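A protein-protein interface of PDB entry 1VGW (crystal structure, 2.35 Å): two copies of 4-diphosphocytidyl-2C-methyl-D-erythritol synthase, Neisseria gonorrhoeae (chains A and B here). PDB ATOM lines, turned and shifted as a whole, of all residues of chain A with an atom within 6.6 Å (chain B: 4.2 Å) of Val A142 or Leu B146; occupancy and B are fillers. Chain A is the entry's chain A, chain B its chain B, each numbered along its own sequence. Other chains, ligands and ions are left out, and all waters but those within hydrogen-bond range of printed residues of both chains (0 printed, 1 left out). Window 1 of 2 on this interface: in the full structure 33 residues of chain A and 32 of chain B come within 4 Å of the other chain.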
ATOM      1  N   VAL A 140       8.116  16.839  19.589  1.00  0.00           N
ATOM      2  CA  VAL A 140       7.491  17.340  18.361  1.00  0.00           C
ATOM      3  C   VAL A 140       7.145  18.820  18.433  1.00  0.00           C
ATOM      4  O   VAL A 140       6.684  19.370  19.455  1.00  0.00           O
ATOM      5  CB  VAL A 140       6.310  16.493  17.876  1.00  0.00           C
ATOM      6  CG1 VAL A 140       6.375  15.029  18.305  1.00  0.00           C
ATOM      7  CG2 VAL A 140       4.943  17.044  18.143  1.00  0.00           C
ATOM      8  N   PRO A 141       7.466  19.623  17.425  1.00  0.00           N
ATOM      9  CA  PRO A 141       7.205  21.059  17.434  1.00  0.00           C
ATOM     10  C   PRO A 141       5.724  21.396  17.664  1.00  0.00           C
ATOM     11  O   PRO A 141       4.857  20.710  17.127  1.00  0.00           O
ATOM     12  CB  PRO A 141       7.552  21.486  15.984  1.00  0.00           C
ATOM     13  CG  PRO A 141       8.615  20.483  15.597  1.00  0.00           C
ATOM     14  CD  PRO A 141       8.079  19.167  16.147  1.00  0.00           C
ATOM     15  N   VAL A 142       5.410  22.424  18.462  1.00  0.00           N
ATOM     16  CA  VAL A 142       3.992  22.795  18.626  1.00  0.00           C
ATOM     17  C   VAL A 142       3.494  23.352  17.307  1.00  0.00           C
ATOM     18  O   VAL A 142       4.092  24.311  16.776  1.00  0.00           O
ATOM     19  CB  VAL A 142       3.828  23.831  19.759  1.00  0.00           C
ATOM     20  CG1 VAL A 142       2.350  24.154  19.996  1.00  0.00           C
ATOM     21  CG2 VAL A 142       4.427  23.283  21.046  1.00  0.00           C
ATOM     22  N   ALA A 143       2.514  22.732  16.655  1.00  0.00           N
ATOM     23  CA  ALA A 143       2.054  23.235  15.371  1.00  0.00           C
ATOM     24  C   ALA A 143       0.810  24.144  15.448  1.00  0.00           C
ATOM     25  O   ALA A 143       0.718  25.009  14.558  1.00  0.00           O
ATOM     26  CB  ALA A 143       1.827  22.141  14.352  1.00  0.00           C
ATOM     27  N   ASP A 144      -0.019  24.070  16.435  1.00  0.00           N
ATOM     28  CA  ASP A 144      -1.207  24.887  16.604  1.00  0.00           C
ATOM     29  C   ASP A 144      -0.999  26.131  17.468  1.00  0.00           C
ATOM     30  O   ASP A 144      -0.224  26.130  18.425  1.00  0.00           O
ATOM     31  CB  ASP A 144      -2.287  24.024  17.332  1.00  0.00           C
ATOM     32  CG  ASP A 144      -2.808  22.882  16.457  1.00  0.00           C
ATOM     33  OD1 ASP A 144      -3.278  21.880  17.060  1.00  0.00           O
ATOM     34  OD2 ASP A 144      -2.806  23.027  15.208  1.00  0.00           O
ATOM     35  N   THR A 145      -1.791  27.169  17.251  1.00  0.00           N
ATOM     36  CA  THR A 145      -1.791  28.404  18.043  1.00  0.00           C
ATOM     37  C   THR A 145      -2.086  28.016  19.490  1.00  0.00           C
ATOM     38  O   THR A 145      -3.014  27.219  19.646  1.00  0.00           O
ATOM     39  CB  THR A 145      -2.934  29.335  17.575  1.00  0.00           C
ATOM     40  OG1 THR A 145      -2.732  29.836  16.246  1.00  0.00           O
ATOM     41  CG2 THR A 145      -3.025  30.571  18.498  1.00  0.00           C
ATOM     42  N   LEU A 146      -1.387  28.521  20.471  1.00  0.00           N
ATOM     43  CA  LEU A 146      -1.644  28.234  21.866  1.00  0.00           C
ATOM     44  C   LEU A 146      -2.413  29.379  22.538  1.00  0.00           C
ATOM     45  O   LEU A 146      -2.140  30.559  22.284  1.00  0.00           O
ATOM     46  CB  LEU A 146      -0.313  28.068  22.614  1.00  0.00           C
ATOM     47  CG  LEU A 146       0.583  26.895  22.304  1.00  0.00           C
ATOM     48  CD1 LEU A 146       1.943  27.107  23.026  1.00  0.00           C
ATOM     49  CD2 LEU A 146      -0.046  25.593  22.807  1.00  0.00           C
ATOM     50  N   VAL A 158      -0.541  32.625  23.390  1.00  0.00           N
ATOM     51  CA  VAL A 158       0.922  32.611  23.686  1.00  0.00           C
ATOM     52  C   VAL A 158       1.721  32.167  22.481  1.00  0.00           C
ATOM     53  O   VAL A 158       1.327  31.246  21.753  1.00  0.00           O
ATOM     54  CB  VAL A 158       1.305  31.985  24.991  1.00  0.00           C
ATOM     55  CG1 VAL A 158       0.093  31.778  25.925  1.00  0.00           C
ATOM     56  CG2 VAL A 158       2.149  30.741  24.904  1.00  0.00           C
ATOM     57  N   ARG A 160       3.931  30.475  19.909  1.00  0.00           N
ATOM     58  CA  ARG A 160       4.423  29.108  19.834  1.00  0.00           C
ATOM     59  C   ARG A 160       5.799  29.037  19.160  1.00  0.00           C
ATOM     60  O   ARG A 160       6.351  27.966  18.868  1.00  0.00           O
ATOM     61  CB  ARG A 160       3.410  28.223  19.102  1.00  0.00           C
ATOM     62  CG  ARG A 160       3.476  28.428  17.586  1.00  0.00           C
ATOM     63  CD  ARG A 160       2.501  27.428  16.912  1.00  0.00           C
ATOM     64  NE  ARG A 160       2.112  28.034  15.639  1.00  0.00           N
ATOM     65  CZ  ARG A 160       2.752  27.830  14.515  1.00  0.00           C
ATOM     66  NH1 ARG A 160       3.800  27.000  14.475  1.00  0.00           N
ATOM     67  NH2 ARG A 160       2.350  28.460  13.433  1.00  0.00           N
ATOM     68  N   GLY A 162       9.428  28.440  18.352  1.00  0.00           N
ATOM     69  CA  GLY A 162      10.484  27.626  18.932  1.00  0.00           C
ATOM     70  C   GLY A 162      10.076  26.754  20.094  1.00  0.00           C
ATOM     71  O   GLY A 162      10.955  26.396  20.909  1.00  0.00           O
ATOM     72  N   LEU A 163       8.793  26.470  20.286  1.00  0.00           N
ATOM     73  CA  LEU A 163       8.291  25.624  21.342  1.00  0.00           C
ATOM     74  C   LEU A 163       8.077  24.186  20.862  1.00  0.00           C
ATOM     75  O   LEU A 163       7.725  23.878  19.717  1.00  0.00           O
ATOM     76  CB  LEU A 163       6.979  26.142  21.964  1.00  0.00           C
ATOM     77  CG  LEU A 163       7.042  27.483  22.691  1.00  0.00           C
ATOM     78  CD1 LEU A 163       5.731  27.823  23.377  1.00  0.00           C
ATOM     79  CD2 LEU A 163       8.116  27.401  23.812  1.00  0.00           C
ATOM     80  N   TRP A 164       8.332  23.240  21.754  1.00  0.00           N
ATOM     81  CA  TRP A 164       8.217  21.815  21.424  1.00  0.00           C
ATOM     82  C   TRP A 164       7.485  21.108  22.571  1.00  0.00           C
ATOM     83  O   TRP A 164       7.618  21.503  23.730  1.00  0.00           O
ATOM     84  CB  TRP A 164       9.635  21.231  21.244  1.00  0.00           C
ATOM     85  CG  TRP A 164      10.478  21.641  20.088  1.00  0.00           C
ATOM     86  CD1 TRP A 164      11.017  22.886  19.869  1.00  0.00           C
ATOM     87  CD2 TRP A 164      11.020  20.828  19.024  1.00  0.00           C
ATOM     88  NE1 TRP A 164      11.790  22.913  18.732  1.00  0.00           N
ATOM     89  CE2 TRP A 164      11.809  21.647  18.201  1.00  0.00           C
ATOM     90  CE3 TRP A 164      10.900  19.484  18.681  1.00  0.00           C
ATOM     91  CZ2 TRP A 164      12.494  21.177  17.079  1.00  0.00           C
ATOM     92  CZ3 TRP A 164      11.561  19.010  17.559  1.00  0.00           C
ATOM     93  CH2 TRP A 164      12.369  19.843  16.770  1.00  0.00           C
ATOM     94  N   GLN A 165       6.734  20.059  22.263  1.00  0.00           N
ATOM     95  CA  GLN A 165       6.087  19.214  23.257  1.00  0.00           C
ATOM     96  C   GLN A 165       6.946  17.941  23.423  1.00  0.00           C
ATOM     97  O   GLN A 165       7.166  17.252  22.431  1.00  0.00           O
ATOM     98  CB  GLN A 165       4.700  18.769  22.781  1.00  0.00           C
ATOM     99  CG  GLN A 165       3.771  19.995  22.662  1.00  0.00           C
ATOM    100  CD  GLN A 165       2.343  19.542  22.408  1.00  0.00           C
ATOM    101  OE1 GLN A 165       1.589  19.330  23.364  1.00  0.00           O
ATOM    102  NE2 GLN A 165       2.043  19.346  21.126  1.00  0.00           N
ATOM    103  N   ALA A 166       7.355  17.646  24.642  1.00  0.00           N
ATOM    104  CA  ALA A 166       8.182  16.498  24.932  1.00  0.00           C
ATOM    105  C   ALA A 166       7.476  15.159  24.917  1.00  0.00           C
ATOM    106  O   ALA A 166       6.297  15.037  25.338  1.00  0.00           O
ATOM    107  CB  ALA A 166       8.785  16.715  26.350  1.00  0.00           C
ATOM    108  N   VAL B 142      -3.032  21.371  26.706  1.00  0.00           N
ATOM    109  CA  VAL B 142      -1.672  20.886  26.428  1.00  0.00           C
ATOM    110  C   VAL B 142      -1.291  19.866  27.493  1.00  0.00           C
ATOM    111  O   VAL B 142      -1.174  20.238  28.646  1.00  0.00           O
ATOM    112  CB  VAL B 142      -0.659  22.037  26.484  1.00  0.00           C
ATOM    113  CG1 VAL B 142       0.777  21.486  26.347  1.00  0.00           C
ATOM    114  CG2 VAL B 142      -0.920  23.038  25.354  1.00  0.00           C
ATOM    115  N   ASP B 144       1.494  17.479  27.484  1.00  0.00           N
ATOM    116  CA  ASP B 144       2.924  17.187  27.669  1.00  0.00           C
ATOM    117  C   ASP B 144       3.739  18.395  28.112  1.00  0.00           C
ATOM    118  O   ASP B 144       3.429  19.529  27.723  1.00  0.00           O
ATOM    119  CB  ASP B 144       3.504  16.724  26.299  1.00  0.00           C
ATOM    120  CG  ASP B 144       3.029  15.365  25.849  1.00  0.00           C
ATOM    121  OD1 ASP B 144       2.965  15.147  24.612  1.00  0.00           O
ATOM    122  OD2 ASP B 144       2.717  14.500  26.715  1.00  0.00           O
ATOM    123  N   THR B 145       4.872  18.203  28.776  1.00  0.00           N
ATOM    124  CA  THR B 145       5.785  19.295  29.135  1.00  0.00           C
ATOM    125  C   THR B 145       6.280  20.059  27.908  1.00  0.00           C
ATOM    126  O   THR B 145       6.695  19.443  26.926  1.00  0.00           O
ATOM    127  CB  THR B 145       7.027  18.701  29.849  1.00  0.00           C
ATOM    128  OG1 THR B 145       6.593  18.052  31.057  1.00  0.00           O
ATOM    129  CG2 THR B 145       8.070  19.758  30.138  1.00  0.00           C
ATOM    130  N   LEU B 146       6.260  21.383  27.947  1.00  0.00           N
ATOM    131  CA  LEU B 146       6.677  22.238  26.850  1.00  0.00           C
ATOM    132  C   LEU B 146       8.132  22.703  27.065  1.00  0.00           C
ATOM    133  O   LEU B 146       8.526  23.055  28.157  1.00  0.00           O
ATOM    134  CB  LEU B 146       5.810  23.485  26.708  1.00  0.00           C
ATOM    135  CG  LEU B 146       4.365  23.399  26.301  1.00  0.00           C
ATOM    136  CD1 LEU B 146       3.675  24.769  26.451  1.00  0.00           C
ATOM    137  CD2 LEU B 146       4.218  22.948  24.841  1.00  0.00           C
ATOM    138  N   LYS B 147       8.891  22.755  25.970  1.00  0.00           N
ATOM    139  CA  LYS B 147      10.259  23.203  26.023  1.00  0.00           C
ATOM    140  C   LYS B 147      10.472  24.305  24.973  1.00  0.00           C
ATOM    141  O   LYS B 147       9.840  24.264  23.932  1.00  0.00           O
ATOM    142  CB  LYS B 147      11.255  22.056  25.735  1.00  0.00           C
ATOM    143  CG  LYS B 147      11.040  20.729  26.434  1.00  0.00           C
ATOM    144  CD  LYS B 147      11.209  20.775  27.945  1.00  0.00           C
ATOM    145  CE  LYS B 147      11.614  19.471  28.554  1.00  0.00           C
ATOM    146  NZ  LYS B 147      11.735  19.402  30.018  1.00  0.00           N
ATOM    147  N   THR B 157      12.307  25.171  30.120  1.00  0.00           N
ATOM    148  CA  THR B 157      11.043  24.416  30.209  1.00  0.00           C
ATOM    149  C   THR B 157       9.946  25.482  30.424  1.00  0.00           C
ATOM    150  O   THR B 157      10.076  26.288  31.369  1.00  0.00           O
ATOM    151  CB  THR B 157      11.101  23.456  31.404  1.00  0.00           C
ATOM    152  OG1 THR B 157      11.812  22.263  30.992  1.00  0.00           O
ATOM    153  CG2 THR B 157       9.735  23.074  31.909  1.00  0.00           C
ATOM    154  N   VAL B 158       8.912  25.537  29.595  1.00  0.00           N
ATOM    155  CA  VAL B 158       7.857  26.540  29.784  1.00  0.00           C
ATOM    156  C   VAL B 158       6.610  25.951  30.401  1.00  0.00           C
ATOM    157  O   VAL B 158       6.115  24.885  30.091  1.00  0.00           O
ATOM    158  CB  VAL B 158       7.651  27.453  28.598  1.00  0.00           C
ATOM    159  CG1 VAL B 158       8.133  26.853  27.303  1.00  0.00           C
ATOM    160  CG2 VAL B 158       6.205  27.910  28.437  1.00  0.00           C
ATOM    161  N   LEU B 163      -2.781  25.965  29.763  1.00  0.00           N
ATOM    162  CA  LEU B 163      -2.580  26.155  28.343  1.00  0.00           C
ATOM    163  C   LEU B 163      -3.339  25.136  27.482  1.00  0.00           C
ATOM    164  O   LEU B 163      -3.636  24.035  27.954  1.00  0.00           O
ATOM    165  CB  LEU B 163      -1.114  26.140  27.916  1.00  0.00           C
ATOM    166  CG  LEU B 163      -0.140  27.121  28.554  1.00  0.00           C
ATOM    167  CD1 LEU B 163       1.137  27.261  27.719  1.00  0.00           C
ATOM    168  CD2 LEU B 163      -0.801  28.515  28.734  1.00  0.00           C
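N of Trp A164 lies within hydrogen-bond range of O of Lys B147. O of Ala A166 sits close to OD1 of Asp B144 (3.4 Å). N of Ala A166 is in hydrogen-bond range of O of Thr B145, 3.0 Å away.
Val A142 touches one residue of chain B. Of chain A, only Val A142, Trp A164 and Gln A165 come within 4 Å of Leu B146. Of the printed residues of chain B, Ala A166 touches Asp B144 and Thr B145. Of the printed residues of chain B, Leu A146 touches Val B142. Arg A160 touches none of the printed residues of chain B. Thr B157 touches none of the printed residues of chain A.
Among the printed residues, merely in contact across the chains: Val A142 with Leu B146 (3.8 Å), Leu A146 with Val B142 (3.7 Å), Gly A162 with Lys B147 (3.9 Å), Leu A163 with Lys B147 (3.3 Å), Leu A163 with Val B158 (3.5 Å), Trp A164 with Thr B145 (3.9 Å), Trp A164 with Leu B146 (3.3 Å), Gln A165 with Val B142 (3.8 Å), Gln A165 with Thr B145 (3.7 Å) and Gln A165 with Leu B146 (3.7 Å).
Of the 14 printed residues of chain A, 7 touch a printed residue of chain B.
Val A142 touches Leu B146, and with the chains exchanged Leu A146 touches Val B142. Leu A163 touches Val B158, but with the chains exchanged Val A158 does not touch Leu B163 (4.4 Å). Positions printed for both chains: 142, 144, 145, 146, 158 and 163.
NZ of Lys B147 is in hydrogen-bond range of OG1 of Thr B157 (3.0 Å). The backbone carbonyl oxygen of Leu B146 sits at hydrogen-bond distance from the backbone NH of Val B158, 2.9 Å away. The backbone carbonyl oxygen (O) of Leu A146 lies within hydrogen-bond range of the backbone NH (N) of Val A158. N of Val A142 sits at hydrogen-bond distance from O of Leu A163. N of Val B142 lies within hydrogen-bond range of O of Leu B163, at 3.0 Å. The backbone carbonyl oxygen (O) of Val A140 sits at hydrogen-bond distance from the backbone NH (N) of Gln A165 (2.9 Å).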
